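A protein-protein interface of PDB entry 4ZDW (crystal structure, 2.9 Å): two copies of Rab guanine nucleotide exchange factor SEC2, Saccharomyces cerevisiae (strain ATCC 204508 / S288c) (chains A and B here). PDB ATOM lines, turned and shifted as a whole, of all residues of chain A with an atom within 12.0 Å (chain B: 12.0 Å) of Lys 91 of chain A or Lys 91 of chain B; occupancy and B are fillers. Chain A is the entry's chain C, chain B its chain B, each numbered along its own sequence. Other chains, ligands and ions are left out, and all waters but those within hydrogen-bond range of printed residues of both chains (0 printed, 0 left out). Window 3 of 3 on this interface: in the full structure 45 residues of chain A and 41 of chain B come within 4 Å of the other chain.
Of the 10 printed residues of chain B, 5 touch a printed residue of chain A.
Of the 10 printed residues of chain A, 5 touch a printed residue of chain B.
Hydrophobic or aromatic side chains of chain A within 4 Å of the printed part of chain B: Leu 84 and Leu 88.
Among the printed residues, 7 pairs touch across the chains.
Lys 82 of chain A touches none of the printed residues of chain B.
Arg 83 of chain A touches none of the printed residues of chain B.
Of the printed residues of chain B, Leu 84 of chain A touches Leu 84 (3.3 Å) and Thr 85 (3.4 Å).
Of the printed residues of chain B, Thr 85 of chain A touches Leu 84 (3.7 Å).
Of the printed residues of chain B, Gln 87 of chain A touches Leu 88.
Of chain B, only Gln 87 and Leu 88 come within 4 Å of Leu 88 of chain A.
No residue of chain B comes within 4 Å of Glu 90 of chain A.
Lys 91 of chain A touches just one residue of chain B: Lys 91 (3.4 Å).
Of the printed residues of chain A, Thr 85 of chain B touches Leu 84.
Leu 88 of chain B touches just these residues of chain A: Gln 87 (3.2 Å) and Leu 88 (3.8 Å).
No residue of chain A comes within 4 Å of Glu 90 of chain B.
Printed residues of chain A within 4 Å of Lys 91 of chain B: Lys 91.
Leu 84 of chain A touches its own counterpart, Leu 84 of chain B.
Leu 84 of chain A touches Thr 85 of chain B, and with the chains exchanged Thr 85 of chain A touches Leu 84 of chain B.
Gln 87 of chain A touches Leu 88 of chain B, and with the chains exchanged Leu 88 of chain A touches Gln 87 of chain B.
Leu 88 of chain B touches its own counterpart, Leu 88 of chain A.
10 positions are printed for both chains.
Among the printed residues, pairs that only touch across the chains: Gln 87 of chain A with Leu 88 of chain B, Leu 84 of chain A with Leu 84 of chain B, Lys 91 of chain A with Lys 91 of chain B, Leu 84 of chain A with Thr 85 of chain B, Leu 88 of chain A with Gln 87 of chain B, Thr 85 of chain A with Leu 84 of chain B and Leu 88 of chain A with Leu 88 of chain B.
The side-chain amide nitrogen (NE2) of Gln 87 of chain A lies close to the guanidinium group (NE) of Arg 83 of chain A.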
ATOM      1  N   LYS A  82     -18.104  21.081 -19.951  1.00  0.00           N
ATOM      2  CA  LYS A  82     -16.906  21.511 -20.662  1.00  0.00           C
ATOM      3  C   LYS A  82     -15.685  21.143 -19.864  1.00  0.00           C
ATOM      4  O   LYS A  82     -14.808  20.430 -20.365  1.00  0.00           O
ATOM      5  CB  LYS A  82     -16.917  23.004 -20.910  1.00  0.00           C
ATOM      6  CG  LYS A  82     -16.972  23.365 -22.383  1.00  0.00           C
ATOM      7  CD  LYS A  82     -17.243  24.849 -22.570  1.00  0.00           C
ATOM      8  CE  LYS A  82     -18.618  25.215 -22.010  1.00  0.00           C
ATOM      9  NZ  LYS A  82     -19.050  26.601 -22.350  1.00  0.00           N
ATOM     10  N   ARG A  83     -15.642  21.604 -18.613  1.00  0.00           N
ATOM     11  CA  ARG A  83     -14.570  21.234 -17.704  1.00  0.00           C
ATOM     12  C   ARG A  83     -14.175  19.754 -17.812  1.00  0.00           C
ATOM     13  O   ARG A  83     -12.997  19.420 -17.732  1.00  0.00           O
ATOM     14  CB  ARG A  83     -14.918  21.605 -16.265  1.00  0.00           C
ATOM     15  CG  ARG A  83     -14.056  20.890 -15.236  1.00  0.00           C
ATOM     16  CD  ARG A  83     -13.368  21.866 -14.292  1.00  0.00           C
ATOM     17  NE  ARG A  83     -11.971  21.477 -14.046  1.00  0.00           N
ATOM     18  CZ  ARG A  83     -11.053  22.255 -13.465  1.00  0.00           C
ATOM     19  NH1 ARG A  83     -11.376  23.481 -13.054  1.00  0.00           N
ATOM     20  NH2 ARG A  83      -9.807  21.812 -13.300  1.00  0.00           N
ATOM     21  N   LEU A  84     -15.140  18.870 -18.021  1.00  0.00           N
ATOM     22  CA  LEU A  84     -14.805  17.455 -18.132  1.00  0.00           C
ATOM     23  C   LEU A  84     -14.247  17.074 -19.497  1.00  0.00           C
ATOM     24  O   LEU A  84     -13.348  16.247 -19.576  1.00  0.00           O
ATOM     25  CB  LEU A  84     -15.983  16.547 -17.771  1.00  0.00           C
ATOM     26  CG  LEU A  84     -16.957  16.743 -16.588  1.00  0.00           C
ATOM     27  CD1 LEU A  84     -17.589  15.393 -16.287  1.00  0.00           C
ATOM     28  CD2 LEU A  84     -16.374  17.358 -15.306  1.00  0.00           C
ATOM     29  N   THR A  85     -14.775  17.658 -20.572  1.00  0.00           N
ATOM     30  CA  THR A  85     -14.277  17.346 -21.917  1.00  0.00           C
ATOM     31  C   THR A  85     -12.880  17.898 -22.103  1.00  0.00           C
ATOM     32  O   THR A  85     -12.076  17.350 -22.871  1.00  0.00           O
ATOM     33  CB  THR A  85     -15.187  17.894 -23.024  1.00  0.00           C
ATOM     34  OG1 THR A  85     -16.468  17.284 -22.902  1.00  0.00           O
ATOM     35  CG2 THR A  85     -14.637  17.560 -24.411  1.00  0.00           C
ATOM     36  N   GLU A  86     -12.589  18.979 -21.388  1.00  0.00           N
ATOM     37  CA  GLU A  86     -11.246  19.525 -21.379  1.00  0.00           C
ATOM     38  C   GLU A  86     -10.245  18.574 -20.691  1.00  0.00           C
ATOM     39  O   GLU A  86      -9.037  18.733 -20.828  1.00  0.00           O
ATOM     40  CB  GLU A  86     -11.236  20.902 -20.715  1.00  0.00           C
ATOM     41  CG  GLU A  86     -10.954  20.849 -19.220  1.00  0.00           C
ATOM     42  CD  GLU A  86     -10.485  22.177 -18.659  1.00  0.00           C
ATOM     43  OE1 GLU A  86     -10.824  23.231 -19.246  1.00  0.00           O
ATOM     44  OE2 GLU A  86      -9.781  22.153 -17.622  1.00  0.00           O
ATOM     45  N   GLN A  87     -10.744  17.593 -19.947  1.00  0.00           N
ATOM     46  CA  GLN A  87      -9.868  16.618 -19.315  1.00  0.00           C
ATOM     47  C   GLN A  87      -9.807  15.346 -20.111  1.00  0.00           C
ATOM     48  O   GLN A  87      -8.822  14.617 -20.048  1.00  0.00           O
ATOM     49  CB  GLN A  87     -10.336  16.313 -17.917  1.00  0.00           C
ATOM     50  CG  GLN A  87     -10.320  17.546 -17.056  1.00  0.00           C
ATOM     51  CD  GLN A  87     -11.150  17.360 -15.824  1.00  0.00           C
ATOM     52  OE1 GLN A  87     -11.608  16.247 -15.533  1.00  0.00           O
ATOM     53  NE2 GLN A  87     -11.361  18.448 -15.082  1.00  0.00           N
ATOM     54  N   LEU A  88     -10.873  15.085 -20.855  1.00  0.00           N
ATOM     55  CA  LEU A  88     -10.877  14.003 -21.821  1.00  0.00           C
ATOM     56  C   LEU A  88      -9.833  14.205 -22.905  1.00  0.00           C
ATOM     57  O   LEU A  88      -9.295  13.229 -23.416  1.00  0.00           O
ATOM     58  CB  LEU A  88     -12.255  13.828 -22.469  1.00  0.00           C
ATOM     59  CG  LEU A  88     -13.366  13.064 -21.738  1.00  0.00           C
ATOM     60  CD1 LEU A  88     -14.055  12.169 -22.759  1.00  0.00           C
ATOM     61  CD2 LEU A  88     -12.871  12.236 -20.548  1.00  0.00           C
ATOM     62  N   ARG A  89      -9.543  15.454 -23.265  1.00  0.00           N
ATOM     63  CA  ARG A  89      -8.526  15.691 -24.289  1.00  0.00           C
ATOM     64  C   ARG A  89      -7.086  15.448 -23.790  1.00  0.00           C
ATOM     65  O   ARG A  89      -6.231  14.959 -24.548  1.00  0.00           O
ATOM     66  CB  ARG A  89      -8.688  17.060 -24.969  1.00  0.00           C
ATOM     67  CG  ARG A  89      -8.825  18.247 -24.035  1.00  0.00           C
ATOM     68  CD  ARG A  89      -8.268  19.520 -24.668  1.00  0.00           C
ATOM     69  NE  ARG A  89      -8.154  20.618 -23.701  1.00  0.00           N
ATOM     70  CZ  ARG A  89      -7.179  20.746 -22.796  1.00  0.00           C
ATOM     71  NH1 ARG A  89      -6.204  19.845 -22.707  1.00  0.00           N
ATOM     72  NH2 ARG A  89      -7.184  21.781 -21.966  1.00  0.00           N
ATOM     73  N   GLU A  90      -6.838  15.761 -22.515  1.00  0.00           N
ATOM     74  CA  GLU A  90      -5.524  15.542 -21.893  1.00  0.00           C
ATOM     75  C   GLU A  90      -5.072  14.087 -21.989  1.00  0.00           C
ATOM     76  O   GLU A  90      -4.088  13.789 -22.672  1.00  0.00           O
ATOM     77  CB  GLU A  90      -5.539  15.994 -20.438  1.00  0.00           C
ATOM     78  CG  GLU A  90      -5.624  17.497 -20.284  1.00  0.00           C
ATOM     79  CD  GLU A  90      -6.398  17.905 -19.051  1.00  0.00           C
ATOM     80  OE1 GLU A  90      -6.657  17.029 -18.192  1.00  0.00           O
ATOM     81  OE2 GLU A  90      -6.750  19.101 -18.946  1.00  0.00           O
ATOM     82  N   LYS A  91      -5.794  13.201 -21.296  1.00  0.00           N
ATOM     83  CA  LYS A  91      -5.592  11.746 -21.373  1.00  0.00           C
ATOM     84  C   LYS A  91      -4.754  11.324 -22.591  1.00  0.00           C
ATOM     85  O   LYS A  91      -3.747  10.619 -22.458  1.00  0.00           O
ATOM     86  CB  LYS A  91      -6.951  11.022 -21.403  1.00  0.00           C
ATOM     87  CG  LYS A  91      -7.406  10.608 -22.803  1.00  0.00           C
ATOM     88  CD  LYS A  91      -8.791   9.976 -22.799  1.00  0.00           C
ATOM     89  CE  LYS A  91      -8.889   8.775 -23.740  1.00  0.00           C
ATOM     90  NZ  LYS A  91      -8.767   9.115 -25.185  1.00  0.00           N
ATOM     91  N   LYS B  82     -23.577  12.819 -17.056  1.00  0.00           N
ATOM     92  CA  LYS B  82     -23.390  11.424 -16.642  1.00  0.00           C
ATOM     93  C   LYS B  82     -22.389  10.692 -17.535  1.00  0.00           C
ATOM     94  O   LYS B  82     -21.349  10.226 -17.058  1.00  0.00           O
ATOM     95  CB  LYS B  82     -24.721  10.653 -16.625  1.00  0.00           C
ATOM     96  CG  LYS B  82     -25.420  10.624 -15.267  1.00  0.00           C
ATOM     97  CD  LYS B  82     -26.947  10.464 -15.353  1.00  0.00           C
ATOM     98  CE  LYS B  82     -27.607  11.044 -14.099  1.00  0.00           C
ATOM     99  NZ  LYS B  82     -29.042  11.393 -14.241  1.00  0.00           N
ATOM    100  N   ARG B  83     -22.689  10.625 -18.834  1.00  0.00           N
ATOM    101  CA  ARG B  83     -21.951   9.744 -19.738  1.00  0.00           C
ATOM    102  C   ARG B  83     -20.499  10.076 -19.834  1.00  0.00           C
ATOM    103  O   ARG B  83     -19.680   9.190 -20.011  1.00  0.00           O
ATOM    104  CB  ARG B  83     -22.530   9.711 -21.141  1.00  0.00           C
ATOM    105  CG  ARG B  83     -22.088   8.475 -21.900  1.00  0.00           C
ATOM    106  CD  ARG B  83     -22.265   8.670 -23.384  1.00  0.00           C
ATOM    107  NE  ARG B  83     -22.037   7.427 -24.133  1.00  0.00           N
ATOM    108  CZ  ARG B  83     -22.468   7.192 -25.383  1.00  0.00           C
ATOM    109  NH1 ARG B  83     -23.178   8.115 -26.047  1.00  0.00           N
ATOM    110  NH2 ARG B  83     -22.197   6.019 -25.973  1.00  0.00           N
ATOM    111  N   LEU B  84     -20.165  11.346 -19.739  1.00  0.00           N
ATOM    112  CA  LEU B  84     -18.762  11.675 -19.749  1.00  0.00           C
ATOM    113  C   LEU B  84     -18.155  11.841 -18.368  1.00  0.00           C
ATOM    114  O   LEU B  84     -16.940  11.890 -18.268  1.00  0.00           O
ATOM    115  CB  LEU B  84     -18.425  12.838 -20.691  1.00  0.00           C
ATOM    116  CG  LEU B  84     -19.066  14.218 -20.606  1.00  0.00           C
ATOM    117  CD1 LEU B  84     -18.303  15.122 -19.654  1.00  0.00           C
ATOM    118  CD2 LEU B  84     -19.101  14.826 -21.999  1.00  0.00           C
ATOM    119  N   THR B  85     -18.962  11.888 -17.305  1.00  0.00           N
ATOM    120  CA  THR B  85     -18.374  11.815 -15.962  1.00  0.00           C
ATOM    121  C   THR B  85     -17.930  10.390 -15.751  1.00  0.00           C
ATOM    122  O   THR B  85     -17.057  10.118 -14.923  1.00  0.00           O
ATOM    123  CB  THR B  85     -19.303  12.218 -14.807  1.00  0.00           C
ATOM    124  OG1 THR B  85     -20.111  13.324 -15.198  1.00  0.00           O
ATOM    125  CG2 THR B  85     -18.484  12.641 -13.584  1.00  0.00           C
ATOM    126  N   GLU B  86     -18.511   9.489 -16.530  1.00  0.00           N
ATOM    127  CA  GLU B  86     -18.156   8.092 -16.435  1.00  0.00           C
ATOM    128  C   GLU B  86     -17.236   7.605 -17.591  1.00  0.00           C
ATOM    129  O   GLU B  86     -16.619   6.543 -17.494  1.00  0.00           O
ATOM    130  CB  GLU B  86     -19.426   7.264 -16.200  1.00  0.00           C
ATOM    131  CG  GLU B  86     -19.221   5.765 -16.087  1.00  0.00           C
ATOM    132  CD  GLU B  86     -19.254   5.084 -17.450  1.00  0.00           C
ATOM    133  OE1 GLU B  86     -19.678   5.748 -18.438  1.00  0.00           O
ATOM    134  OE2 GLU B  86     -18.850   3.894 -17.527  1.00  0.00           O
ATOM    135  N   GLN B  87     -17.126   8.391 -18.664  1.00  0.00           N
ATOM    136  CA  GLN B  87     -16.152   8.117 -19.735  1.00  0.00           C
ATOM    137  C   GLN B  87     -14.778   8.384 -19.193  1.00  0.00           C
ATOM    138  O   GLN B  87     -13.846   7.628 -19.448  1.00  0.00           O
ATOM    139  CB  GLN B  87     -16.374   9.017 -20.951  1.00  0.00           C
ATOM    140  CG  GLN B  87     -17.192   8.381 -22.080  1.00  0.00           C
ATOM    141  CD  GLN B  87     -17.531   9.356 -23.212  1.00  0.00           C
ATOM    142  OE1 GLN B  87     -17.012  10.476 -23.273  1.00  0.00           O
ATOM    143  NE2 GLN B  87     -18.406   8.927 -24.118  1.00  0.00           N
ATOM    144  N   LEU B  88     -14.662   9.476 -18.444  1.00  0.00           N
ATOM    145  CA  LEU B  88     -13.470   9.738 -17.668  1.00  0.00           C
ATOM    146  C   LEU B  88     -13.281   8.653 -16.597  1.00  0.00           C
ATOM    147  O   LEU B  88     -12.233   8.014 -16.547  1.00  0.00           O
ATOM    148  CB  LEU B  88     -13.542  11.123 -17.016  1.00  0.00           C
ATOM    149  CG  LEU B  88     -12.299  11.641 -16.279  1.00  0.00           C
ATOM    150  CD1 LEU B  88     -12.364  13.167 -16.160  1.00  0.00           C
ATOM    151  CD2 LEU B  88     -12.116  10.967 -14.912  1.00  0.00           C
ATOM    152  N   ARG B  89     -14.301   8.437 -15.764  1.00  0.00           N
ATOM    153  CA  ARG B  89     -14.146   7.663 -14.517  1.00  0.00           C
ATOM    154  C   ARG B  89     -13.399   6.342 -14.584  1.00  0.00           C
ATOM    155  O   ARG B  89     -12.306   6.227 -14.015  1.00  0.00           O
ATOM    156  CB  ARG B  89     -15.469   7.493 -13.772  1.00  0.00           C
ATOM    157  CG  ARG B  89     -15.736   8.678 -12.870  1.00  0.00           C
ATOM    158  CD  ARG B  89     -16.895   8.469 -11.904  1.00  0.00           C
ATOM    159  NE  ARG B  89     -17.152   9.698 -11.146  1.00  0.00           N
ATOM    160  CZ  ARG B  89     -16.316  10.245 -10.257  1.00  0.00           C
ATOM    161  NH1 ARG B  89     -15.134   9.688  -9.985  1.00  0.00           N
ATOM    162  NH2 ARG B  89     -16.663  11.365  -9.636  1.00  0.00           N
ATOM    163  N   GLU B  90     -13.975   5.353 -15.270  1.00  0.00           N
ATOM    164  CA  GLU B  90     -13.325   4.040 -15.400  1.00  0.00           C
ATOM    165  C   GLU B  90     -11.890   4.170 -15.993  1.00  0.00           C
ATOM    166  O   GLU B  90     -11.032   3.291 -15.799  1.00  0.00           O
ATOM    167  CB  GLU B  90     -14.233   3.058 -16.184  1.00  0.00           C
ATOM    168  CG  GLU B  90     -13.814   2.693 -17.612  1.00  0.00           C
ATOM    169  CD  GLU B  90     -13.728   3.880 -18.566  1.00  0.00           C
ATOM    170  OE1 GLU B  90     -14.540   4.824 -18.439  1.00  0.00           O
ATOM    171  OE2 GLU B  90     -12.836   3.864 -19.447  1.00  0.00           O
ATOM    172  N   LYS B  91     -11.651   5.304 -16.665  1.00  0.00           N
ATOM    173  CA  LYS B  91     -10.445   5.566 -17.458  1.00  0.00           C
ATOM    174  C   LYS B  91      -9.523   6.615 -16.805  1.00  0.00           C
ATOM    175  O   LYS B  91      -8.765   6.322 -15.875  1.00  0.00           O
ATOM    176  CB  LYS B  91     -10.872   6.057 -18.845  1.00  0.00           C
ATOM    177  CG  LYS B  91      -9.965   5.625 -19.979  1.00  0.00           C
ATOM    178  CD  LYS B  91      -9.639   6.799 -20.887  1.00  0.00           C
ATOM    179  CE  LYS B  91      -8.511   7.650 -20.308  1.00  0.00           C
ATOM    180  NZ  LYS B  91      -8.956   8.593 -19.239  1.00  0.00           N
